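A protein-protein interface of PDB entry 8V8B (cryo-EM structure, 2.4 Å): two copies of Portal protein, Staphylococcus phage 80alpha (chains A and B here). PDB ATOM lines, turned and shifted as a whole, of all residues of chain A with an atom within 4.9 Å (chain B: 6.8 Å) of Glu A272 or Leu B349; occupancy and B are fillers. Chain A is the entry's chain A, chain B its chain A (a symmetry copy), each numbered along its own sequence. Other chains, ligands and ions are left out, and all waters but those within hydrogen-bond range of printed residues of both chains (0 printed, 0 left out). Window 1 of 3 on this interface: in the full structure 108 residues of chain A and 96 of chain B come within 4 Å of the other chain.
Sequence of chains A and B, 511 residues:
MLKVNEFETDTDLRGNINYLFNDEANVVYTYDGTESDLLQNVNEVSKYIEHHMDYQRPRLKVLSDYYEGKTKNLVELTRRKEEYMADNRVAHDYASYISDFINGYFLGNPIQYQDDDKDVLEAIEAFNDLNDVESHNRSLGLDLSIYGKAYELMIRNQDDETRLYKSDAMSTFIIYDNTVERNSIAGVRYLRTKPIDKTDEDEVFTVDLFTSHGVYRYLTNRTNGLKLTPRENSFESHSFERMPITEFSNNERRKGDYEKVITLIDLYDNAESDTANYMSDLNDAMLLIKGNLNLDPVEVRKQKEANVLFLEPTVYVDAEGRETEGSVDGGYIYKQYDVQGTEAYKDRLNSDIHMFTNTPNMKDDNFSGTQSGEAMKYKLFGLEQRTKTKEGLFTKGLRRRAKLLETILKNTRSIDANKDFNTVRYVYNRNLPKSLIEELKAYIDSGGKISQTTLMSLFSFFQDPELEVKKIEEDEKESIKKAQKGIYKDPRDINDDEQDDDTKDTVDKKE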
ATOM      1  N   VAL A  90     -23.595  17.283 -11.507  1.00  0.00           N
ATOM      2  CA  VAL A  90     -24.409  17.774 -10.396  1.00  0.00           C
ATOM      3  C   VAL A  90     -25.777  18.222 -10.910  1.00  0.00           C
ATOM      4  O   VAL A  90     -25.909  18.674 -12.045  1.00  0.00           O
ATOM      5  CB  VAL A  90     -23.673  18.912  -9.644  1.00  0.00           C
ATOM      6  CG1 VAL A  90     -23.579  20.166 -10.500  1.00  0.00           C
ATOM      7  CG2 VAL A  90     -24.345  19.208  -8.306  1.00  0.00           C
ATOM      8  N   HIS A  92     -29.242  20.557  -9.407  1.00  0.00           N
ATOM      9  CA  HIS A  92     -29.839  21.394  -8.365  1.00  0.00           C
ATOM     10  C   HIS A  92     -31.362  21.336  -8.395  1.00  0.00           C
ATOM     11  O   HIS A  92     -31.978  21.471  -9.453  1.00  0.00           O
ATOM     12  CB  HIS A  92     -29.353  22.839  -8.460  1.00  0.00           C
ATOM     13  CG  HIS A  92     -27.897  22.992  -8.159  1.00  0.00           C
ATOM     14  ND1 HIS A  92     -26.906  22.668  -9.059  1.00  0.00           N
ATOM     15  CD2 HIS A  92     -27.264  23.404  -7.038  1.00  0.00           C
ATOM     16  CE1 HIS A  92     -25.728  22.887  -8.508  1.00  0.00           C
ATOM     17  NE2 HIS A  92     -25.918  23.331  -7.282  1.00  0.00           N
ATOM     18  N   TYR A 268     -26.640  27.118 -13.557  1.00  0.00           N
ATOM     19  CA  TYR A 268     -26.223  26.898 -12.185  1.00  0.00           C
ATOM     20  C   TYR A 268     -25.592  25.519 -11.993  1.00  0.00           C
ATOM     21  O   TYR A 268     -24.614  25.396 -11.253  1.00  0.00           O
ATOM     22  CB  TYR A 268     -27.406  27.116 -11.245  1.00  0.00           C
ATOM     23  CG  TYR A 268     -27.016  27.410  -9.813  1.00  0.00           C
ATOM     24  CD1 TYR A 268     -26.786  28.713  -9.392  1.00  0.00           C
ATOM     25  CD2 TYR A 268     -26.959  26.402  -8.864  1.00  0.00           C
ATOM     26  CE1 TYR A 268     -26.448  28.991  -8.088  1.00  0.00           C
ATOM     27  CE2 TYR A 268     -26.618  26.671  -7.555  1.00  0.00           C
ATOM     28  CZ  TYR A 268     -26.368  27.969  -7.171  1.00  0.00           C
ATOM     29  OH  TYR A 268     -26.044  28.248  -5.870  1.00  0.00           O
ATOM     30  N   ASP A 269     -26.107  24.473 -12.652  1.00  0.00           N
ATOM     31  CA  ASP A 269     -25.386  23.194 -12.664  1.00  0.00           C
ATOM     32  C   ASP A 269     -23.980  23.278 -13.267  1.00  0.00           C
ATOM     33  O   ASP A 269     -22.990  22.954 -12.595  1.00  0.00           O
ATOM     34  CB  ASP A 269     -26.197  22.133 -13.415  1.00  0.00           C
ATOM     35  CG  ASP A 269     -27.458  21.717 -12.686  1.00  0.00           C
ATOM     36  OD1 ASP A 269     -27.582  21.989 -11.481  1.00  0.00           O
ATOM     37  OD2 ASP A 269     -28.322  21.095 -13.316  1.00  0.00           O
ATOM     38  N   ASN A 270     -23.846  23.900 -14.439  1.00  0.00           N
ATOM     39  CA  ASN A 270     -22.520  24.021 -15.046  1.00  0.00           C
ATOM     40  C   ASN A 270     -21.538  24.754 -14.148  1.00  0.00           C
ATOM     41  O   ASN A 270     -20.450  24.242 -13.865  1.00  0.00           O
ATOM     42  CB  ASN A 270     -22.614  24.678 -16.422  1.00  0.00           C
ATOM     43  CG  ASN A 270     -23.408  23.854 -17.407  1.00  0.00           C
ATOM     44  OD1 ASN A 270     -23.839  22.752 -17.102  1.00  0.00           O
ATOM     45  ND2 ASN A 270     -23.585  24.374 -18.601  1.00  0.00           N
ATOM     46  N   ALA A 271     -21.911  25.935 -13.667  1.00  0.00           N
ATOM     47  CA  ALA A 271     -21.035  26.684 -12.779  1.00  0.00           C
ATOM     48  C   ALA A 271     -20.453  25.797 -11.683  1.00  0.00           C
ATOM     49  O   ALA A 271     -19.227  25.679 -11.561  1.00  0.00           O
ATOM     50  CB  ALA A 271     -21.788  27.872 -12.175  1.00  0.00           C
ATOM     51  N   GLU A 272     -21.297  25.039 -10.979  1.00  0.00           N
ATOM     52  CA  GLU A 272     -20.737  24.241  -9.895  1.00  0.00           C
ATOM     53  C   GLU A 272     -19.882  23.096 -10.410  1.00  0.00           C
ATOM     54  O   GLU A 272     -18.763  22.901  -9.924  1.00  0.00           O
ATOM     55  CB  GLU A 272     -21.845  23.699  -8.984  1.00  0.00           C
ATOM     56  CG  GLU A 272     -22.606  24.730  -8.174  1.00  0.00           C
ATOM     57  CD  GLU A 272     -21.736  25.479  -7.177  1.00  0.00           C
ATOM     58  OE1 GLU A 272     -20.772  26.139  -7.600  1.00  0.00           O
ATOM     59  OE2 GLU A 272     -22.026  25.425  -5.966  1.00  0.00           O
ATOM     60  N   SER A 273     -20.318  22.399 -11.455  1.00  0.00           N
ATOM     61  CA  SER A 273     -19.458  21.330 -11.940  1.00  0.00           C
ATOM     62  C   SER A 273     -18.152  21.868 -12.507  1.00  0.00           C
ATOM     63  O   SER A 273     -17.154  21.148 -12.503  1.00  0.00           O
ATOM     64  CB  SER A 273     -20.180  20.436 -12.952  1.00  0.00           C
ATOM     65  OG  SER A 273     -20.847  21.164 -13.945  1.00  0.00           O
ATOM     66  N   ASP A 274     -18.117  23.111 -13.005  1.00  0.00           N
ATOM     67  CA  ASP A 274     -16.817  23.670 -13.373  1.00  0.00           C
ATOM     68  C   ASP A 274     -15.891  23.883 -12.182  1.00  0.00           C
ATOM     69  O   ASP A 274     -14.735  23.448 -12.216  1.00  0.00           O
ATOM     70  CB  ASP A 274     -16.984  24.972 -14.154  1.00  0.00           C
ATOM     71  CG  ASP A 274     -17.699  24.777 -15.470  1.00  0.00           C
ATOM     72  OD1 ASP A 274     -17.935  23.618 -15.866  1.00  0.00           O
ATOM     73  OD2 ASP A 274     -18.030  25.786 -16.116  1.00  0.00           O
ATOM     74  N   THR A 275     -16.413  24.413 -11.077  1.00  0.00           N
ATOM     75  CA  THR A 275     -15.582  24.608  -9.893  1.00  0.00           C
ATOM     76  C   THR A 275     -15.030  23.294  -9.378  1.00  0.00           C
ATOM     77  O   THR A 275     -13.817  23.152  -9.180  1.00  0.00           O
ATOM     78  CB  THR A 275     -16.378  25.343  -8.809  1.00  0.00           C
ATOM     79  OG1 THR A 275     -17.150  26.383  -9.413  1.00  0.00           O
ATOM     80  CG2 THR A 275     -15.482  25.936  -7.747  1.00  0.00           C
ATOM     81  N   ALA A 276     -15.890  22.297  -9.218  1.00  0.00           N
ATOM     82  CA  ALA A 276     -15.415  20.980  -8.831  1.00  0.00           C
ATOM     83  C   ALA A 276     -14.304  20.476  -9.751  1.00  0.00           C
ATOM     84  O   ALA A 276     -13.217  20.115  -9.279  1.00  0.00           O
ATOM     85  CB  ALA A 276     -16.592  20.005  -8.821  1.00  0.00           C
ATOM     86  N   LYS A 346     -22.471  33.221  -9.447  1.00  0.00           N
ATOM     87  CA  LYS A 346     -23.374  32.254  -8.823  1.00  0.00           C
ATOM     88  C   LYS A 346     -24.474  32.893  -7.973  1.00  0.00           C
ATOM     89  O   LYS A 346     -25.626  32.455  -8.034  1.00  0.00           O
ATOM     90  CB  LYS A 346     -22.598  31.209  -8.025  1.00  0.00           C
ATOM     91  CG  LYS A 346     -21.528  30.527  -8.830  1.00  0.00           C
ATOM     92  CD  LYS A 346     -20.622  29.667  -8.003  1.00  0.00           C
ATOM     93  CE  LYS A 346     -19.491  29.147  -8.847  1.00  0.00           C
ATOM     94  NZ  LYS A 346     -18.658  28.180  -8.112  1.00  0.00           N
ATOM     95  N   TYR B  94     -25.106  14.192   5.738  1.00  0.00           N
ATOM     96  CA  TYR B  94     -26.285  15.027   5.509  1.00  0.00           C
ATOM     97  C   TYR B  94     -27.591  14.242   5.516  1.00  0.00           C
ATOM     98  O   TYR B  94     -28.597  14.718   6.050  1.00  0.00           O
ATOM     99  CB  TYR B  94     -26.173  15.755   4.174  1.00  0.00           C
ATOM    100  CG  TYR B  94     -25.195  16.883   4.122  1.00  0.00           C
ATOM    101  CD1 TYR B  94     -25.496  18.100   4.700  1.00  0.00           C
ATOM    102  CD2 TYR B  94     -24.004  16.761   3.435  1.00  0.00           C
ATOM    103  CE1 TYR B  94     -24.624  19.140   4.651  1.00  0.00           C
ATOM    104  CE2 TYR B  94     -23.124  17.801   3.376  1.00  0.00           C
ATOM    105  CZ  TYR B  94     -23.441  18.990   3.984  1.00  0.00           C
ATOM    106  OH  TYR B  94     -22.584  20.044   3.909  1.00  0.00           O
ATOM    107  N   THR B 263     -26.301  14.123  -5.377  1.00  0.00           N
ATOM    108  CA  THR B 263     -25.170  14.652  -6.148  1.00  0.00           C
ATOM    109  C   THR B 263     -24.474  15.845  -5.491  1.00  0.00           C
ATOM    110  O   THR B 263     -23.239  15.879  -5.446  1.00  0.00           O
ATOM    111  CB  THR B 263     -25.583  14.989  -7.596  1.00  0.00           C
ATOM    112  OG1 THR B 263     -26.300  16.226  -7.650  1.00  0.00           O
ATOM    113  CG2 THR B 263     -26.360  13.872  -8.246  1.00  0.00           C
ATOM    114  N   LEU B 264     -25.215  16.741  -4.839  1.00  0.00           N
ATOM    115  CA  LEU B 264     -24.547  17.781  -4.052  1.00  0.00           C
ATOM    116  C   LEU B 264     -23.686  17.175  -2.959  1.00  0.00           C
ATOM    117  O   LEU B 264     -22.521  17.545  -2.808  1.00  0.00           O
ATOM    118  CB  LEU B 264     -25.539  18.785  -3.460  1.00  0.00           C
ATOM    119  CG  LEU B 264     -26.480  19.530  -4.399  1.00  0.00           C
ATOM    120  CD1 LEU B 264     -27.513  20.328  -3.639  1.00  0.00           C
ATOM    121  CD2 LEU B 264     -25.669  20.455  -5.252  1.00  0.00           C
ATOM    122  N   ILE B 265     -24.253  16.282  -2.153  1.00  0.00           N
ATOM    123  CA  ILE B 265     -23.456  15.604  -1.138  1.00  0.00           C
ATOM    124  C   ILE B 265     -22.166  15.030  -1.733  1.00  0.00           C
ATOM    125  O   ILE B 265     -21.073  15.243  -1.191  1.00  0.00           O
ATOM    126  CB  ILE B 265     -24.301  14.506  -0.451  1.00  0.00           C
ATOM    127  CG1 ILE B 265     -25.520  15.125   0.242  1.00  0.00           C
ATOM    128  CG2 ILE B 265     -23.455  13.674   0.505  1.00  0.00           C
ATOM    129  CD1 ILE B 265     -26.545  14.124   0.771  1.00  0.00           C
ATOM    130  N   LEU B 267     -20.463  16.158  -4.416  1.00  0.00           N
ATOM    131  CA  LEU B 267     -19.559  17.295  -4.557  1.00  0.00           C
ATOM    132  C   LEU B 267     -18.938  17.677  -3.228  1.00  0.00           C
ATOM    133  O   LEU B 267     -17.719  17.845  -3.132  1.00  0.00           O
ATOM    134  CB  LEU B 267     -20.240  18.504  -5.210  1.00  0.00           C
ATOM    135  CG  LEU B 267     -20.681  18.379  -6.674  1.00  0.00           C
ATOM    136  CD1 LEU B 267     -21.060  19.738  -7.225  1.00  0.00           C
ATOM    137  CD2 LEU B 267     -19.600  17.777  -7.540  1.00  0.00           C
ATOM    138  N   TYR B 268     -19.754  17.826  -2.191  1.00  0.00           N
ATOM    139  CA  TYR B 268     -19.204  18.233  -0.912  1.00  0.00           C
ATOM    140  C   TYR B 268     -18.155  17.246  -0.400  1.00  0.00           C
ATOM    141  O   TYR B 268     -17.145  17.670   0.164  1.00  0.00           O
ATOM    142  CB  TYR B 268     -20.334  18.433   0.096  1.00  0.00           C
ATOM    143  CG  TYR B 268     -19.970  19.312   1.271  1.00  0.00           C
ATOM    144  CD1 TYR B 268     -20.143  20.688   1.210  1.00  0.00           C
ATOM    145  CD2 TYR B 268     -19.535  18.764   2.469  1.00  0.00           C
ATOM    146  CE1 TYR B 268     -19.830  21.494   2.281  1.00  0.00           C
ATOM    147  CE2 TYR B 268     -19.217  19.565   3.546  1.00  0.00           C
ATOM    148  CZ  TYR B 268     -19.372  20.929   3.448  1.00  0.00           C
ATOM    149  OH  TYR B 268     -19.073  21.731   4.518  1.00  0.00           O
ATOM    150  N   ASP B 269     -18.349  15.935  -0.594  1.00  0.00           N
ATOM    151  CA  ASP B 269     -17.260  14.989  -0.320  1.00  0.00           C
ATOM    152  C   ASP B 269     -15.995  15.242  -1.147  1.00  0.00           C
ATOM    153  O   ASP B 269     -14.914  15.466  -0.583  1.00  0.00           O
ATOM    154  CB  ASP B 269     -17.734  13.551  -0.545  1.00  0.00           C
ATOM    155  CG  ASP B 269     -18.749  13.088   0.480  1.00  0.00           C
ATOM    156  OD1 ASP B 269     -18.879  13.724   1.538  1.00  0.00           O
ATOM    157  OD2 ASP B 269     -19.407  12.068   0.237  1.00  0.00           O
ATOM    158  N   ALA B 271     -14.911  18.045  -2.715  1.00  0.00           N
ATOM    159  CA  ALA B 271     -14.267  19.273  -2.274  1.00  0.00           C
ATOM    160  C   ALA B 271     -13.365  19.033  -1.067  1.00  0.00           C
ATOM    161  O   ALA B 271     -12.161  19.311  -1.123  1.00  0.00           O
ATOM    162  CB  ALA B 271     -15.320  20.339  -1.962  1.00  0.00           C
ATOM    163  N   ALA B 344     -15.729  29.791   0.053  1.00  0.00           N
ATOM    164  CA  ALA B 344     -17.051  30.246  -0.360  1.00  0.00           C
ATOM    165  C   ALA B 344     -17.805  29.218  -1.199  1.00  0.00           C
ATOM    166  O   ALA B 344     -18.986  28.955  -0.944  1.00  0.00           O
ATOM    167  CB  ALA B 344     -16.922  31.555  -1.112  1.00  0.00           C
ATOM    168  N   TYR B 345     -17.131  28.560  -2.144  1.00  0.00           N
ATOM    169  CA  TYR B 345     -17.770  27.461  -2.868  1.00  0.00           C
ATOM    170  C   TYR B 345     -18.330  26.404  -1.915  1.00  0.00           C
ATOM    171  O   TYR B 345     -19.523  26.083  -1.963  1.00  0.00           O
ATOM    172  CB  TYR B 345     -16.781  26.870  -3.881  1.00  0.00           C
ATOM    173  CG  TYR B 345     -17.140  25.521  -4.454  1.00  0.00           C
ATOM    174  CD1 TYR B 345     -18.244  25.347  -5.272  1.00  0.00           C
ATOM    175  CD2 TYR B 345     -16.306  24.432  -4.247  1.00  0.00           C
ATOM    176  CE1 TYR B 345     -18.539  24.120  -5.807  1.00  0.00           C
ATOM    177  CE2 TYR B 345     -16.594  23.208  -4.774  1.00  0.00           C
ATOM    178  CZ  TYR B 345     -17.708  23.056  -5.560  1.00  0.00           C
ATOM    179  OH  TYR B 345     -17.994  21.822  -6.077  1.00  0.00           O
ATOM    180  N   LYS B 346     -17.504  25.892  -1.006  1.00  0.00           N
ATOM    181  CA  LYS B 346     -18.010  24.999   0.037  1.00  0.00           C
ATOM    182  C   LYS B 346     -19.202  25.564   0.812  1.00  0.00           C
ATOM    183  O   LYS B 346     -20.155  24.833   1.089  1.00  0.00           O
ATOM    184  CB  LYS B 346     -16.893  24.566   0.983  1.00  0.00           C
ATOM    185  CG  LYS B 346     -15.714  23.968   0.268  1.00  0.00           C
ATOM    186  CD  LYS B 346     -14.531  23.746   1.162  1.00  0.00           C
ATOM    187  CE  LYS B 346     -13.348  23.296   0.348  1.00  0.00           C
ATOM    188  NZ  LYS B 346     -12.206  22.926   1.201  1.00  0.00           N
ATOM    189  N   ASP B 347     -19.147  26.827   1.250  1.00  0.00           N
ATOM    190  CA  ASP B 347     -20.358  27.442   1.800  1.00  0.00           C
ATOM    191  C   ASP B 347     -21.588  27.241   0.917  1.00  0.00           C
ATOM    192  O   ASP B 347     -22.582  26.642   1.343  1.00  0.00           O
ATOM    193  CB  ASP B 347     -20.144  28.936   2.048  1.00  0.00           C
ATOM    194  CG  ASP B 347     -19.336  29.219   3.282  1.00  0.00           C
ATOM    195  OD1 ASP B 347     -19.196  28.324   4.136  1.00  0.00           O
ATOM    196  OD2 ASP B 347     -18.820  30.347   3.398  1.00  0.00           O
ATOM    197  N   ARG B 348     -21.494  27.640  -0.346  1.00  0.00           N
ATOM    198  CA  ARG B 348     -22.624  27.525  -1.256  1.00  0.00           C
ATOM    199  C   ARG B 348     -23.235  26.127  -1.242  1.00  0.00           C
ATOM    200  O   ARG B 348     -24.397  25.952  -0.868  1.00  0.00           O
ATOM    201  CB  ARG B 348     -22.171  27.925  -2.656  1.00  0.00           C
ATOM    202  CG  ARG B 348     -23.270  27.971  -3.669  1.00  0.00           C
ATOM    203  CD  ARG B 348     -22.808  28.610  -4.962  1.00  0.00           C
ATOM    204  NE  ARG B 348     -22.487  30.025  -4.824  1.00  0.00           N
ATOM    205  CZ  ARG B 348     -23.375  30.983  -4.604  1.00  0.00           C
ATOM    206  NH1 ARG B 348     -24.667  30.790  -4.813  1.00  0.00           N
ATOM    207  NH2 ARG B 348     -22.950  32.196  -4.279  1.00  0.00           N
ATOM    208  N   LEU B 349     -22.441  25.112  -1.578  1.00  0.00           N
ATOM    209  CA  LEU B 349     -22.912  23.735  -1.518  1.00  0.00           C
ATOM    210  C   LEU B 349     -23.687  23.439  -0.241  1.00  0.00           C
ATOM    211  O   LEU B 349     -24.865  23.064  -0.287  1.00  0.00           O
ATOM    212  CB  LEU B 349     -21.739  22.755  -1.658  1.00  0.00           C
ATOM    213  CG  LEU B 349     -21.010  22.686  -2.999  1.00  0.00           C
ATOM    214  CD1 LEU B 349     -19.698  21.952  -2.840  1.00  0.00           C
ATOM    215  CD2 LEU B 349     -21.871  22.029  -4.064  1.00  0.00           C
ATOM    216  N   ASN B 350     -23.046  23.632   0.911  1.00  0.00           N
ATOM    217  CA  ASN B 350     -23.728  23.415   2.180  1.00  0.00           C
ATOM    218  C   ASN B 350     -25.112  24.064   2.184  1.00  0.00           C
ATOM    219  O   ASN B 350     -26.138  23.377   2.258  1.00  0.00           O
ATOM    220  CB  ASN B 350     -22.843  23.931   3.325  1.00  0.00           C
ATOM    221  CG  ASN B 350     -23.484  23.776   4.697  1.00  0.00           C
ATOM    222  OD1 ASN B 350     -23.695  22.669   5.160  1.00  0.00           O
ATOM    223  ND2 ASN B 350     -23.785  24.887   5.348  1.00  0.00           N
ATOM    224  N   SER B 351     -25.161  25.380   1.998  1.00  0.00           N
ATOM    225  CA  SER B 351     -26.446  26.065   2.031  1.00  0.00           C
ATOM    226  C   SER B 351     -27.452  25.481   1.037  1.00  0.00           C
ATOM    227  O   SER B 351     -28.595  25.198   1.417  1.00  0.00           O
ATOM    228  CB  SER B 351     -26.249  27.569   1.823  1.00  0.00           C
ATOM    229  OG  SER B 351     -25.770  27.885   0.543  1.00  0.00           O
ATOM    230  N   ASP B 352     -27.034  25.195  -0.204  1.00  0.00           N
ATOM    231  CA  ASP B 352     -27.965  24.574  -1.147  1.00  0.00           C
ATOM    232  C   ASP B 352     -28.569  23.288  -0.608  1.00  0.00           C
ATOM    233  O   ASP B 352     -29.794  23.129  -0.625  1.00  0.00           O
ATOM    234  CB  ASP B 352     -27.316  24.335  -2.509  1.00  0.00           C
ATOM    235  CG  ASP B 352     -26.762  25.605  -3.127  1.00  0.00           C
ATOM    236  OD1 ASP B 352     -27.218  26.696  -2.734  1.00  0.00           O
ATOM    237  OD2 ASP B 352     -25.903  25.522  -4.028  1.00  0.00           O
ATOM    238  N   ILE B 353     -27.747  22.353  -0.135  1.00  0.00           N
ATOM    239  CA  ILE B 353     -28.302  21.168   0.515  1.00  0.00           C
ATOM    240  C   ILE B 353     -29.414  21.533   1.494  1.00  0.00           C
ATOM    241  O   ILE B 353     -30.527  21.019   1.376  1.00  0.00           O
ATOM    242  CB  ILE B 353     -27.222  20.272   1.165  1.00  0.00           C
ATOM    243  CG1 ILE B 353     -26.136  19.895   0.146  1.00  0.00           C
ATOM    244  CG2 ILE B 353     -27.827  19.018   1.762  1.00  0.00           C
ATOM    245  CD1 ILE B 353     -24.805  19.526   0.734  1.00  0.00           C
ATOM    246  N   HIS B 354     -29.128  22.380   2.481  1.00  0.00           N
ATOM    247  CA  HIS B 354     -30.181  22.806   3.403  1.00  0.00           C
ATOM    248  C   HIS B 354     -31.360  23.487   2.714  1.00  0.00           C
ATOM    249  O   HIS B 354     -32.516  23.147   2.988  1.00  0.00           O
ATOM    250  CB  HIS B 354     -29.601  23.670   4.523  1.00  0.00           C
ATOM    251  CG  HIS B 354     -28.579  22.961   5.351  1.00  0.00           C
ATOM    252  ND1 HIS B 354     -27.298  23.428   5.534  1.00  0.00           N
ATOM    253  CD2 HIS B 354     -28.663  21.812   6.059  1.00  0.00           C
ATOM    254  CE1 HIS B 354     -26.635  22.592   6.311  1.00  0.00           C
ATOM    255  NE2 HIS B 354     -27.441  21.604   6.642  1.00  0.00           N
ATOM    256  N   MET B 355     -31.106  24.381   1.763  1.00  0.00           N
ATOM    257  CA  MET B 355     -32.217  25.117   1.165  1.00  0.00           C
ATOM    258  C   MET B 355     -33.194  24.208   0.429  1.00  0.00           C
ATOM    259  O   MET B 355     -34.409  24.359   0.572  1.00  0.00           O
ATOM    260  CB  MET B 355     -31.687  26.213   0.242  1.00  0.00           C
ATOM    261  CG  MET B 355     -32.731  27.260  -0.131  1.00  0.00           C
ATOM    262  SD  MET B 355     -33.498  28.127   1.268  1.00  0.00           S
ATOM    263  CE  MET B 355     -32.225  29.278   1.776  1.00  0.00           C
ATOM    264  N   ASN B 361     -29.922  25.883   8.559  1.00  0.00           N
ATOM    265  CA  ASN B 361     -28.589  26.098   8.007  1.00  0.00           C
ATOM    266  C   ASN B 361     -27.643  26.908   8.885  1.00  0.00           C
ATOM    267  O   ASN B 361     -26.434  26.723   8.779  1.00  0.00           O
ATOM    268  CB  ASN B 361     -28.692  26.794   6.646  1.00  0.00           C
ATOM    269  CG  ASN B 361     -27.372  26.823   5.899  1.00  0.00           C
ATOM    270  OD1 ASN B 361     -26.898  25.806   5.407  1.00  0.00           O
ATOM    271  ND2 ASN B 361     -26.812  28.006   5.751  1.00  0.00           N
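Glu A272 touches just these residues of chain B: Tyr B345 (3.5 Å), Arg B348 (3.4 Å) and Leu B349 (3.9 Å).
Of chain A, only Glu A272 (3.9 Å) comes within 4 Å of Leu B349.
Of the printed residues of chain A, Asp B352 touches His A92 (3.9 Å) and Tyr A268 (3.3 Å).
Printed residues of chain A within 4 Å of Leu B267: Val A90 and Ala A276.
Of the printed residues of chain B, Val A90 touches Thr B263, Leu B264 and Leu B267.
The nearest printed residue of chain A that does not touch Leu B267 is Glu A272 (4.4 Å).
Of the 21 printed residues of chain B, 7 touch a printed residue of chain A.
Hydrophobic or aromatic side chains of chain B within 4 Å of the printed part of chain A: Leu B264, Leu B267, Tyr B345 and Leu B349.
Along chain B the printed residues that touch a printed residue of chain A span positions 263 to 352.
Printed residues of chain A that touch a printed residue of chain B: Val A90, His A92, Tyr A268, Glu A272, Thr A275, Ala A276 and Lys A346.
Among the printed residues, no Asp or Glu carboxylate lies within 4 Å of a Lys or Arg side-chain nitrogen of the other chain.
Positions printed for both chains: 268, 269, 271 and 346.
The side-chain hydroxyl (OH) of Tyr A268 sits at hydrogen-bond distance from the guanidinium group (NH1) of Arg B348 (3.1 Å).
The side-chain hydroxyl of Tyr A268 is in hydrogen-bond range of the side-chain carboxylate of Asp B352.
Among the printed residues, merely in contact across the chains: Val A90 with Thr B263 (3.6 Å), Val A90 with Leu B264 (3.6 Å), Val A90 with Leu B267 (3.5 Å), His A92 with Leu B264 (3.5 Å), His A92 with Asp B352 (3.9 Å), Glu A272 with Tyr B345 (3.5 Å), Glu A272 with Arg B348 (3.4 Å), Glu A272 with Leu B349 (3.9 Å), Thr A275 with Tyr B345 (3.7 Å), Ala A276 with Leu B267 (3.96 Å), Ala A276 with Tyr B345 (3.6 Å) and Lys A346 with Arg B348 (3.4 Å).
A ring nitrogen (ND1) of His A92 is in hydrogen-bond range of the side-chain carboxylate (OD1) of Asp A269 (2.6 Å).
The backbone carbonyl oxygen (O) of Ala A271 is in hydrogen-bond range of the side-chain hydroxyl (OG1) of Thr A275 (3.1 Å).
The side-chain amino group of Lys A346 lies within salt-bridge range of the side-chain carboxylate of Glu A272, at 3.0 Å.
OG1 of Thr A275 is in hydrogen-bond range of NZ of Lys A346, 2.7 Å away.
The backbone carbonyl oxygen (O) of Arg B348 is in hydrogen-bond range of the side-chain hydroxyl (OG) of Ser B351.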
